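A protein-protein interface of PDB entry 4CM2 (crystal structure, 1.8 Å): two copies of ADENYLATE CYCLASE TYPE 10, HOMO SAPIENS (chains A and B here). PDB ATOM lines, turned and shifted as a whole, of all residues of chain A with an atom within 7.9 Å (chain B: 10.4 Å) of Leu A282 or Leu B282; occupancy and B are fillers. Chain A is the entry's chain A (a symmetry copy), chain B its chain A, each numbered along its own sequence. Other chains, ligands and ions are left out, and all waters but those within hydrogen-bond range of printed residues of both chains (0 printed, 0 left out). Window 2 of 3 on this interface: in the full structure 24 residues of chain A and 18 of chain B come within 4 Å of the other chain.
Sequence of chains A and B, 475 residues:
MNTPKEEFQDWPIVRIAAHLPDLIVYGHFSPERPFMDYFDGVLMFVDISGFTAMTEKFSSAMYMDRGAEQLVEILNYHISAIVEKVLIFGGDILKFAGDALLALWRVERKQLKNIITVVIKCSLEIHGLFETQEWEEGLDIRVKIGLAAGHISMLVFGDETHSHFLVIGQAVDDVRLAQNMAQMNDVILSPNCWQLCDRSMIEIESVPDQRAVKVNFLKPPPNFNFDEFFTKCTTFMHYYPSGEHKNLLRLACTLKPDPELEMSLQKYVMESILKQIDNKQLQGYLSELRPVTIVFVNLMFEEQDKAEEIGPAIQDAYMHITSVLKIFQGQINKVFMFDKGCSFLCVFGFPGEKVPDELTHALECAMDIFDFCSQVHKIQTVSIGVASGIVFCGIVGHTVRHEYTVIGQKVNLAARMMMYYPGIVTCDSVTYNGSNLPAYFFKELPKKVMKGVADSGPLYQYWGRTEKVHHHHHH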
ATOM      1  N   SER A 272       4.594  42.983  39.533  1.00  0.00           N
ATOM      2  CA  SER A 272       4.787  41.948  38.533  1.00  0.00           C
ATOM      3  C   SER A 272       6.259  41.518  38.443  1.00  0.00           C
ATOM      4  O   SER A 272       6.515  40.378  38.115  1.00  0.00           O
ATOM      5  CB  SER A 272       4.298  42.452  37.151  1.00  0.00           C
ATOM      6  OG  SER A 272       4.961  43.649  36.803  1.00  0.00           O
ATOM      7  N   LYS A 275       6.755  39.117  41.255  1.00  0.00           N
ATOM      8  CA  LYS A 275       6.140  37.809  40.889  1.00  0.00           C
ATOM      9  C   LYS A 275       7.122  36.905  40.134  1.00  0.00           C
ATOM     10  O   LYS A 275       7.313  35.727  40.461  1.00  0.00           O
ATOM     11  CB  LYS A 275       4.863  38.031  40.064  1.00  0.00           C
ATOM     12  CG  LYS A 275       3.919  36.859  40.131  1.00  0.00           C
ATOM     13  CD  LYS A 275       2.670  37.001  39.271  1.00  0.00           C
ATOM     14  CE  LYS A 275       1.785  35.791  39.461  1.00  0.00           C
ATOM     15  NZ  LYS A 275       0.478  36.091  38.770  1.00  0.00           N
ATOM     16  N   GLN A 276       7.856  37.534  39.223  1.00  0.00           N
ATOM     17  CA  GLN A 276       8.931  36.829  38.490  1.00  0.00           C
ATOM     18  C   GLN A 276      10.025  36.414  39.370  1.00  0.00           C
ATOM     19  O   GLN A 276      10.528  35.273  39.318  1.00  0.00           O
ATOM     20  CB  GLN A 276       9.370  37.713  37.331  1.00  0.00           C
ATOM     21  CG  GLN A 276      10.394  37.080  36.479  1.00  0.00           C
ATOM     22  CD  GLN A 276      10.914  38.058  35.429  1.00  0.00           C
ATOM     23  OE1 GLN A 276      10.115  38.694  34.691  1.00  0.00           O
ATOM     24  NE2 GLN A 276      12.245  38.165  35.354  1.00  0.00           N
ATOM     25  N   ILE A 277      10.448  37.347  40.218  1.00  0.00           N
ATOM     26  CA  ILE A 277      11.537  37.090  41.213  1.00  0.00           C
ATOM     27  C   ILE A 277      11.190  35.910  42.122  1.00  0.00           C
ATOM     28  O   ILE A 277      12.069  35.100  42.460  1.00  0.00           O
ATOM     29  CB  ILE A 277      11.838  38.358  41.986  1.00  0.00           C
ATOM     30  CG1 ILE A 277      12.725  39.304  41.117  1.00  0.00           C
ATOM     31  CG2 ILE A 277      12.549  38.039  43.316  1.00  0.00           C
ATOM     32  CD1 ILE A 277      12.936  40.644  41.699  1.00  0.00           C
ATOM     33  N   ASN A 279       9.599  33.332  41.295  1.00  0.00           N
ATOM     34  CA  ASN A 279       9.312  32.192  40.403  1.00  0.00           C
ATOM     35  C   ASN A 279       7.860  31.825  40.326  1.00  0.00           C
ATOM     36  O   ASN A 279       7.487  30.621  40.269  1.00  0.00           O
ATOM     37  CB  ASN A 279      10.215  31.014  40.839  1.00  0.00           C
ATOM     38  CG  ASN A 279      11.662  31.311  40.699  1.00  0.00           C
ATOM     39  OD1 ASN A 279      12.090  31.978  39.770  1.00  0.00           O
ATOM     40  ND2 ASN A 279      12.449  30.780  41.629  1.00  0.00           N
ATOM     41  N   LYS A 280       6.969  32.830  40.296  1.00  0.00           N
ATOM     42  CA  LYS A 280       5.532  32.652  40.171  1.00  0.00           C
ATOM     43  C   LYS A 280       4.987  33.162  38.861  1.00  0.00           C
ATOM     44  O   LYS A 280       3.809  33.094  38.612  1.00  0.00           O
ATOM     45  CB  LYS A 280       4.762  33.273  41.380  1.00  0.00           C
ATOM     46  CG  LYS A 280       5.021  32.398  42.670  1.00  0.00           C
ATOM     47  CD  LYS A 280       4.112  32.886  43.856  1.00  0.00           C
ATOM     48  CE  LYS A 280       4.045  31.946  45.111  1.00  0.00           C
ATOM     49  NZ  LYS A 280       5.290  31.882  45.833  1.00  0.00           N
ATOM     50  N   GLN A 281       5.925  33.517  37.958  1.00  0.00           N
ATOM     51  CA  GLN A 281       5.628  34.033  36.622  1.00  0.00           C
ATOM     52  C   GLN A 281       6.838  33.644  35.766  1.00  0.00           C
ATOM     53  O   GLN A 281       7.972  33.710  36.252  1.00  0.00           O
ATOM     54  CB  GLN A 281       5.589  35.544  36.683  1.00  0.00           C
ATOM     55  CG  GLN A 281       5.119  36.304  35.479  1.00  0.00           C
ATOM     56  CD  GLN A 281       4.656  37.705  35.900  1.00  0.00           C
ATOM     57  OE1 GLN A 281       3.547  37.823  36.353  1.00  0.00           O
ATOM     58  NE2 GLN A 281       5.550  38.695  35.918  1.00  0.00           N
ATOM     59  N   LEU A 282       6.615  33.317  34.537  1.00  0.00           N
ATOM     60  CA  LEU A 282       7.723  32.990  33.582  1.00  0.00           C
ATOM     61  C   LEU A 282       8.663  34.149  33.357  1.00  0.00           C
ATOM     62  O   LEU A 282       8.247  35.276  33.326  1.00  0.00           O
ATOM     63  CB  LEU A 282       7.070  32.595  32.231  1.00  0.00           C
ATOM     64  CG  LEU A 282       6.233  31.330  32.348  1.00  0.00           C
ATOM     65  CD1 LEU A 282       5.150  31.140  31.239  1.00  0.00           C
ATOM     66  CD2 LEU A 282       7.116  30.119  32.416  1.00  0.00           C
ATOM     67  N   GLN A 283       9.947  33.827  33.212  1.00  0.00           N
ATOM     68  CA  GLN A 283      11.056  34.832  33.248  1.00  0.00           C
ATOM     69  C   GLN A 283      10.992  35.701  32.067  1.00  0.00           C
ATOM     70  O   GLN A 283      11.590  36.770  32.106  1.00  0.00           O
ATOM     71  CB  GLN A 283      12.412  34.214  33.442  1.00  0.00           C
ATOM     72  CG  GLN A 283      12.554  33.457  34.775  1.00  0.00           C
ATOM     73  CD  GLN A 283      12.427  34.310  36.072  1.00  0.00           C
ATOM     74  OE1 GLN A 283      13.112  35.360  36.228  1.00  0.00           O
ATOM     75  NE2 GLN A 283      11.595  33.843  37.023  1.00  0.00           N
ATOM     76  N   GLY A 284      10.268  35.271  31.029  1.00  0.00           N
ATOM     77  CA  GLY A 284      10.135  36.025  29.799  1.00  0.00           C
ATOM     78  C   GLY A 284       8.835  36.755  29.594  1.00  0.00           C
ATOM     79  O   GLY A 284       8.703  37.475  28.634  1.00  0.00           O
ATOM     80  N   TYR A 285       7.912  36.724  30.573  1.00  0.00           N
ATOM     81  CA  TYR A 285       6.612  37.205  30.395  1.00  0.00           C
ATOM     82  C   TYR A 285       6.514  38.768  30.251  1.00  0.00           C
ATOM     83  O   TYR A 285       5.620  39.301  29.649  1.00  0.00           O
ATOM     84  CB  TYR A 285       5.790  36.824  31.676  1.00  0.00           C
ATOM     85  CG  TYR A 285       4.376  37.303  31.714  1.00  0.00           C
ATOM     86  CD1 TYR A 285       3.319  36.567  31.126  1.00  0.00           C
ATOM     87  CD2 TYR A 285       4.063  38.433  32.444  1.00  0.00           C
ATOM     88  CE1 TYR A 285       1.985  37.043  31.238  1.00  0.00           C
ATOM     89  CE2 TYR A 285       2.785  38.892  32.576  1.00  0.00           C
ATOM     90  CZ  TYR A 285       1.747  38.220  31.971  1.00  0.00           C
ATOM     91  OH  TYR A 285       0.529  38.850  32.177  1.00  0.00           O
ATOM     92  N   LEU A 286       7.435  39.455  30.839  1.00  0.00           N
ATOM     93  CA  LEU A 286       7.406  40.925  30.818  1.00  0.00           C
ATOM     94  C   LEU A 286       8.105  41.536  29.593  1.00  0.00           C
ATOM     95  O   LEU A 286       8.022  42.782  29.481  1.00  0.00           O
ATOM     96  CB  LEU A 286       8.059  41.503  32.088  1.00  0.00           C
ATOM     97  CG  LEU A 286       7.241  41.234  33.350  1.00  0.00           C
ATOM     98  CD1 LEU A 286       8.009  41.748  34.553  1.00  0.00           C
ATOM     99  CD2 LEU A 286       5.938  41.978  33.254  1.00  0.00           C
ATOM    100  N   SER A 287       8.713  40.766  28.696  1.00  0.00           N
ATOM    101  CA  SER A 287       9.297  41.300  27.438  1.00  0.00           C
ATOM    102  C   SER A 287       8.209  41.313  26.411  1.00  0.00           C
ATOM    103  O   SER A 287       7.856  40.265  25.917  1.00  0.00           O
ATOM    104  CB  SER A 287      10.485  40.507  26.903  1.00  0.00           C
ATOM    105  OG  SER A 287      11.548  40.600  27.825  1.00  0.00           O
ATOM    106  N   ARG B  15      20.422  29.501  22.180  1.00  0.00           N
ATOM    107  CA  ARG B  15      19.426  28.468  22.395  1.00  0.00           C
ATOM    108  C   ARG B  15      18.792  27.984  21.069  1.00  0.00           C
ATOM    109  O   ARG B  15      18.549  26.796  20.924  1.00  0.00           O
ATOM    110  CB  ARG B  15      18.319  29.002  23.330  1.00  0.00           C
ATOM    111  CG  ARG B  15      18.778  29.299  24.733  1.00  0.00           C
ATOM    112  CD  ARG B  15      17.542  29.841  25.508  1.00  0.00           C
ATOM    113  NE  ARG B  15      17.809  29.863  26.949  1.00  0.00           N
ATOM    114  CZ  ARG B  15      16.871  29.950  27.908  1.00  0.00           C
ATOM    115  NH1 ARG B  15      15.592  30.003  27.603  1.00  0.00           N
ATOM    116  NH2 ARG B  15      17.257  29.883  29.212  1.00  0.00           N
ATOM    117  N   SER B 272       6.379  26.771  18.875  1.00  0.00           N
ATOM    118  CA  SER B 272       6.279  26.396  20.274  1.00  0.00           C
ATOM    119  C   SER B 272       7.664  26.201  20.909  1.00  0.00           C
ATOM    120  O   SER B 272       7.803  26.429  22.091  1.00  0.00           O
ATOM    121  CB  SER B 272       5.446  25.096  20.414  1.00  0.00           C
ATOM    122  OG  SER B 272       6.012  24.065  19.634  1.00  0.00           O
ATOM    123  N   ILE B 273       8.679  25.835  20.139  1.00  0.00           N
ATOM    124  CA  ILE B 273      10.058  25.703  20.708  1.00  0.00           C
ATOM    125  C   ILE B 273      10.583  27.089  20.979  1.00  0.00           C
ATOM    126  O   ILE B 273      11.227  27.338  22.014  1.00  0.00           O
ATOM    127  CB  ILE B 273      11.086  25.005  19.810  1.00  0.00           C
ATOM    128  CG1 ILE B 273      10.677  23.562  19.561  1.00  0.00           C
ATOM    129  CG2 ILE B 273      12.451  24.983  20.519  1.00  0.00           C
ATOM    130  CD1 ILE B 273      11.215  22.632  20.611  1.00  0.00           C
ATOM    131  N   LEU B 274      10.296  28.035  20.037  1.00  0.00           N
ATOM    132  CA  LEU B 274      10.710  29.416  20.205  1.00  0.00           C
ATOM    133  C   LEU B 274      10.053  30.032  21.443  1.00  0.00           C
ATOM    134  O   LEU B 274      10.748  30.751  22.187  1.00  0.00           O
ATOM    135  CB  LEU B 274      10.405  30.260  18.926  1.00  0.00           C
ATOM    136  CG  LEU B 274      11.249  29.844  17.684  1.00  0.00           C
ATOM    137  CD1 LEU B 274      10.671  30.579  16.442  1.00  0.00           C
ATOM    138  CD2 LEU B 274      12.687  30.215  17.838  1.00  0.00           C
ATOM    139  N   LYS B 275       8.854  29.636  21.747  1.00  0.00           N
ATOM    140  CA  LYS B 275       8.140  30.111  22.967  1.00  0.00           C
ATOM    141  C   LYS B 275       8.867  29.701  24.253  1.00  0.00           C
ATOM    142  O   LYS B 275       9.118  30.513  25.152  1.00  0.00           O
ATOM    143  CB  LYS B 275       6.693  29.595  22.973  1.00  0.00           C
ATOM    144  CG  LYS B 275       5.781  30.442  23.822  1.00  0.00           C
ATOM    145  CD  LYS B 275       4.350  29.931  23.920  1.00  0.00           C
ATOM    146  CE  LYS B 275       3.526  30.885  24.753  1.00  0.00           C
ATOM    147  NZ  LYS B 275       2.087  30.451  24.625  1.00  0.00           N
ATOM    148  N   GLN B 276       9.340  28.460  24.242  1.00  0.00           N
ATOM    149  CA  GLN B 276      10.167  27.949  25.359  1.00  0.00           C
ATOM    150  C   GLN B 276      11.450  28.647  25.467  1.00  0.00           C
ATOM    151  O   GLN B 276      11.899  29.052  26.558  1.00  0.00           O
ATOM    152  CB  GLN B 276      10.294  26.440  25.199  1.00  0.00           C
ATOM    153  CG  GLN B 276      11.041  25.806  26.302  1.00  0.00           C
ATOM    154  CD  GLN B 276      11.277  24.324  26.021  1.00  0.00           C
ATOM    155  OE1 GLN B 276      10.321  23.570  25.698  1.00  0.00           O
ATOM    156  NE2 GLN B 276      12.540  23.908  26.160  1.00  0.00           N
ATOM    157  N   ILE B 277      12.101  28.805  24.318  1.00  0.00           N
ATOM    158  CA  ILE B 277      13.412  29.523  24.233  1.00  0.00           C
ATOM    159  C   ILE B 277      13.301  30.945  24.782  1.00  0.00           C
ATOM    160  O   ILE B 277      14.224  31.431  25.456  1.00  0.00           O
ATOM    161  CB  ILE B 277      13.932  29.480  22.811  1.00  0.00           C
ATOM    162  CG1 ILE B 277      14.570  28.083  22.528  1.00  0.00           C
ATOM    163  CG2 ILE B 277      14.968  30.594  22.567  1.00  0.00           C
ATOM    164  CD1 ILE B 277      14.953  27.865  21.119  1.00  0.00           C
ATOM    165  N   ASP B 278      12.158  31.587  24.534  1.00  0.00           N
ATOM    166  CA  ASP B 278      11.915  32.957  25.000  1.00  0.00           C
ATOM    167  C   ASP B 278      11.421  33.012  26.472  1.00  0.00           C
ATOM    168  O   ASP B 278      11.034  34.055  26.985  1.00  0.00           O
ATOM    169  CB  ASP B 278      10.934  33.578  24.043  1.00  0.00           C
ATOM    170  CG  ASP B 278      11.597  33.923  22.668  1.00  0.00           C
ATOM    171  OD1 ASP B 278      12.769  34.297  22.652  1.00  0.00           O
ATOM    172  OD2 ASP B 278      10.811  33.910  21.655  1.00  0.00           O
ATOM    173  N   ASN B 279      11.501  31.878  27.180  1.00  0.00           N
ATOM    174  CA  ASN B 279      10.965  31.755  28.549  1.00  0.00           C
ATOM    175  C   ASN B 279       9.539  32.199  28.691  1.00  0.00           C
ATOM    176  O   ASN B 279       9.143  32.828  29.710  1.00  0.00           O
ATOM    177  CB  ASN B 279      11.930  32.499  29.502  1.00  0.00           C
ATOM    178  CG  ASN B 279      13.292  31.910  29.521  1.00  0.00           C
ATOM    179  OD1 ASN B 279      13.467  30.704  29.442  1.00  0.00           O
ATOM    180  ND2 ASN B 279      14.290  32.775  29.663  1.00  0.00           N
ATOM    181  N   LYS B 280       8.691  31.879  27.700  1.00  0.00           N
ATOM    182  CA  LYS B 280       7.270  32.185  27.702  1.00  0.00           C
ATOM    183  C   LYS B 280       6.402  30.955  27.794  1.00  0.00           C
ATOM    184  O   LYS B 280       5.200  31.044  27.797  1.00  0.00           O
ATOM    185  CB  LYS B 280       6.864  33.068  26.478  1.00  0.00           C
ATOM    186  CG  LYS B 280       7.443  34.525  26.672  1.00  0.00           C
ATOM    187  CD  LYS B 280       6.896  35.487  25.556  1.00  0.00           C
ATOM    188  CE  LYS B 280       7.152  37.021  25.772  1.00  0.00           C
ATOM    189  NZ  LYS B 280       8.543  37.378  25.672  1.00  0.00           N
ATOM    190  N   GLN B 281       7.070  29.810  28.047  1.00  0.00           N
ATOM    191  CA  GLN B 281       6.434  28.500  28.184  1.00  0.00           C
ATOM    192  C   GLN B 281       7.363  27.700  29.103  1.00  0.00           C
ATOM    193  O   GLN B 281       8.587  27.820  28.984  1.00  0.00           O
ATOM    194  CB  GLN B 281       6.441  27.816  26.835  1.00  0.00           C
ATOM    195  CG  GLN B 281       5.677  26.535  26.671  1.00  0.00           C
ATOM    196  CD  GLN B 281       5.370  26.302  25.185  1.00  0.00           C
ATOM    197  OE1 GLN B 281       4.425  26.875  24.707  1.00  0.00           O
ATOM    198  NE2 GLN B 281       6.253  25.630  24.447  1.00  0.00           N
ATOM    199  N   LEU B 282       6.813  26.877  29.933  1.00  0.00           N
ATOM    200  CA  LEU B 282       7.618  25.987  30.830  1.00  0.00           C
ATOM    201  C   LEU B 282       8.484  25.014  30.066  1.00  0.00           C
ATOM    202  O   LEU B 282       8.095  24.527  29.038  1.00  0.00           O
ATOM    203  CB  LEU B 282       6.619  25.192  31.714  1.00  0.00           C
ATOM    204  CG  LEU B 282       5.821  26.103  32.635  1.00  0.00           C
ATOM    205  CD1 LEU B 282       4.478  25.509  33.163  1.00  0.00           C
ATOM    206  CD2 LEU B 282       6.669  26.558  33.787  1.00  0.00           C
ATOM    207  N   GLN B 283       9.675  24.763  30.604  1.00  0.00           N
ATOM    208  CA  GLN B 283      10.771  24.048  29.875  1.00  0.00           C
ATOM    209  C   GLN B 283      10.407  22.641  29.665  1.00  0.00           C
ATOM    210  O   GLN B 283      11.013  22.013  28.805  1.00  0.00           O
ATOM    211  CB  GLN B 283      12.118  24.210  30.521  1.00  0.00           C
ATOM    212  CG  GLN B 283      12.599  25.671  30.574  1.00  0.00           C
ATOM    213  CD  GLN B 283      12.840  26.370  29.202  1.00  0.00           C
ATOM    214  OE1 GLN B 283      13.560  25.829  28.316  1.00  0.00           O
ATOM    215  NE2 GLN B 283      12.286  27.587  29.039  1.00  0.00           N
ATOM    216  N   GLY B 284       9.424  22.144  30.421  1.00  0.00           N
ATOM    217  CA  GLY B 284       8.979  20.768  30.325  1.00  0.00           C
ATOM    218  C   GLY B 284       7.685  20.529  29.594  1.00  0.00           C
ATOM    219  O   GLY B 284       7.313  19.397  29.399  1.00  0.00           O
ATOM    220  N   TYR B 285       7.058  21.575  29.025  1.00  0.00           N
ATOM    221  CA  TYR B 285       5.766  21.481  28.499  1.00  0.00           C
ATOM    222  C   TYR B 285       5.662  20.612  27.192  1.00  0.00           C
ATOM    223  O   TYR B 285       4.649  20.045  26.880  1.00  0.00           O
ATOM    224  CB  TYR B 285       5.312  22.931  28.107  1.00  0.00           C
ATOM    225  CG  TYR B 285       3.969  23.045  27.464  1.00  0.00           C
ATOM    226  CD1 TYR B 285       2.781  23.152  28.226  1.00  0.00           C
ATOM    227  CD2 TYR B 285       3.883  23.172  26.091  1.00  0.00           C
ATOM    228  CE1 TYR B 285       1.534  23.311  27.562  1.00  0.00           C
ATOM    229  CE2 TYR B 285       2.697  23.345  25.441  1.00  0.00           C
ATOM    230  CZ  TYR B 285       1.523  23.402  26.158  1.00  0.00           C
ATOM    231  OH  TYR B 285       0.416  23.538  25.334  1.00  0.00           O
ATOM    232  N   LEU B 286       6.719  20.561  26.454  1.00  0.00           N
ATOM    233  CA  LEU B 286       6.712  19.826  25.180  1.00  0.00           C
ATOM    234  C   LEU B 286       7.067  18.338  25.327  1.00  0.00           C
ATOM    235  O   LEU B 286       6.978  17.648  24.284  1.00  0.00           O
ATOM    236  CB  LEU B 286       7.691  20.461  24.176  1.00  0.00           C
ATOM    237  CG  LEU B 286       7.238  21.839  23.695  1.00  0.00           C
ATOM    238  CD1 LEU B 286       8.310  22.423  22.795  1.00  0.00           C
ATOM    239  CD2 LEU B 286       5.970  21.685  22.901  1.00  0.00           C
ATOM    240  N   SER B 287       7.398  17.826  26.508  1.00  0.00           N
ATOM    241  CA  SER B 287       7.632  16.373  26.722  1.00  0.00           C
ATOM    242  C   SER B 287       6.309  15.748  27.033  1.00  0.00           C
ATOM    243  O   SER B 287       5.818  15.929  28.126  1.00  0.00           O
ATOM    244  CB  SER B 287       8.619  16.048  27.839  1.00  0.00           C
ATOM    245  OG  SER B 287       9.891  16.537  27.481  1.00  0.00           O
ATOM    246  N   GLU B 288       5.745  14.988  26.111  1.00  0.00           N
ATOM    247  CA  GLU B 288       4.397  14.450  26.376  1.00  0.00           C
ATOM    248  C   GLU B 288       4.111  13.237  25.559  1.00  0.00           C
ATOM    249  O   GLU B 288       4.722  12.954  24.548  1.00  0.00           O
ATOM    250  CB  GLU B 288       3.336  15.559  26.132  1.00  0.00           C
ATOM    251  CG  GLU B 288       3.431  16.136  24.771  1.00  0.00           C
ATOM    252  CD  GLU B 288       2.407  17.238  24.510  1.00  0.00           C
ATOM    253  OE1 GLU B 288       1.301  17.205  25.154  1.00  0.00           O
ATOM    254  OE2 GLU B 288       2.750  18.110  23.647  1.00  0.00           O
ATOM    255  N   PRO B 351       2.284  20.583  19.745  1.00  0.00           N
ATOM    256  CA  PRO B 351       2.270  21.671  20.781  1.00  0.00           C
ATOM    257  C   PRO B 351       0.946  22.448  21.004  1.00  0.00           C
ATOM    258  O   PRO B 351       0.835  23.603  20.559  1.00  0.00           O
ATOM    259  CB  PRO B 351       3.344  22.641  20.265  1.00  0.00           C
ATOM    260  CG  PRO B 351       4.267  21.814  19.483  1.00  0.00           C
ATOM    261  CD  PRO B 351       3.616  20.502  19.124  1.00  0.00           C
ATOM    262  N   ILE B 395      11.878  17.247  23.121  1.00  0.00           N
ATOM    263  CA  ILE B 395      13.213  17.662  22.663  1.00  0.00           C
ATOM    264  C   ILE B 395      14.234  16.591  23.063  1.00  0.00           C
ATOM    265  O   ILE B 395      14.498  16.378  24.255  1.00  0.00           O
ATOM    266  CB  ILE B 395      13.616  19.047  23.211  1.00  0.00           C
ATOM    267  CG1 ILE B 395      12.611  20.098  22.662  1.00  0.00           C
ATOM    268  CG2 ILE B 395      15.002  19.386  22.789  1.00  0.00           C
ATOM    269  CD1 ILE B 395      12.684  21.458  23.357  1.00  0.00           C
ATOM    270  N   TYR B 404      13.341  18.728  18.416  1.00  0.00           N
ATOM    271  CA  TYR B 404      12.006  18.228  18.805  1.00  0.00           C
ATOM    272  C   TYR B 404      11.735  17.043  17.903  1.00  0.00           C
ATOM    273  O   TYR B 404      11.875  17.133  16.651  1.00  0.00           O
ATOM    274  CB  TYR B 404      11.033  19.309  18.473  1.00  0.00           C
ATOM    275  CG  TYR B 404       9.653  18.974  18.956  1.00  0.00           C
ATOM    276  CD1 TYR B 404       9.361  18.845  20.320  1.00  0.00           C
ATOM    277  CD2 TYR B 404       8.658  18.732  18.030  1.00  0.00           C
ATOM    278  CE1 TYR B 404       8.067  18.503  20.735  1.00  0.00           C
ATOM    279  CE2 TYR B 404       7.377  18.448  18.462  1.00  0.00           C
ATOM    280  CZ  TYR B 404       7.094  18.363  19.784  1.00  0.00           C
ATOM    281  OH  TYR B 404       5.716  18.057  20.058  1.00  0.00           O
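Hydrophobic or aromatic side chains of chain B that line the printed part of chain A: Leu B282. Of the 13 printed residues of chain A, 4 touch a printed residue of chain B. Hydrophobic or aromatic side chains of chain A within 4 Å of the printed part of chain B: Leu A282. Among the printed residues, no Asp or Glu carboxylate lies within 4 Å of a Lys or Arg side-chain nitrogen of the other chain.
Leu A282 touches Asn B279. Leu A282 touches Lys B280 (CD1 to O, 3.4 Å). Leu A282 touches Gln B281. Leu A282 touches Leu B282 (CD2 to CD2, 3.8 Å). N of Gln A283 touches O of Asn B279, 3.7 Å away. Asp B278 touches Gly A284.
The backbone NH of Gly A284 sits at hydrogen-bond distance from the backbone carbonyl oxygen of Asn B279 (3.0 Å). The backbone carbonyl oxygen of Gly A284 sits at hydrogen-bond distance from the side-chain amino group of Lys B280, 3.0 Å away. O of Ser A287 is in hydrogen-bond range of NZ of Lys B280 (3.0 Å).
NH1 of Arg B15 lies within hydrogen-bond range of OD1 of Asn B279 (2.9 Å). The backbone carbonyl oxygen (O) of Ser B272 lies within hydrogen-bond range of the side-chain amide nitrogen (NE2) of Gln B281 (2.9 Å). O of Lys B275 is in hydrogen-bond range of N of Lys B280. OD1 of Asn B279 sits at hydrogen-bond distance from NE2 of Gln B283. The backbone carbonyl oxygen of Gln A276 sits at hydrogen-bond distance from the side-chain amide nitrogen of Gln A283, 2.9 Å away. The side-chain amide oxygen of Asn A279 lies within hydrogen-bond range of the side-chain amide nitrogen of Gln A283, at 3.4 Å.
Of the printed residues of chain B, Leu A282 touches Asn B279 (3.3 Å), Lys B280 (3.4 Å), Gln B281 (3.96 Å) and Leu B282 (3.8 Å). Of chain B, only Asn B279 comes within 4 Å of Gln A283. Printed residues of chain B within 4 Å of Ser A287: Lys B280. Printed residues of chain A within 4 Å of Asp B278: Gly A284 (3.6 Å). Printed residues of chain A within 4 Å of Asn B279: Leu A282 (3.3 Å), Gln A283 (3.7 Å) and Gly A284 (3.0 Å). Of the printed residues of chain A, Lys B280 touches Leu A282, Gly A284 and Ser A287. Of the printed residues of chain A, Gln B281 touches Leu A282 (3.96 Å). Of chain A, only Leu A282 comes within 4 Å of Leu B282. Glu B288 touches none of the printed residues of chain A. The nearest printed residue of chain A that does not touch Leu B282 is Gln A281 (7.4 Å).
Leu A282 touches Asn B279, but with the chains exchanged Asn A279 does not touch Leu B282 (7.7 Å). Leu A282 touches Lys B280, but with the chains exchanged Lys A280 does not touch Leu B282 (8.5 Å). Leu A282 touches its own counterpart, Leu B282. Ser A287 touches Lys B280, but with the chains exchanged Lys A280 does not touch Ser B287 (19.8 Å). Positions printed for both chains: 272, 275, 276, 277, 279, 280, 281, 282, 283, 284, 285, 286 and 287.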
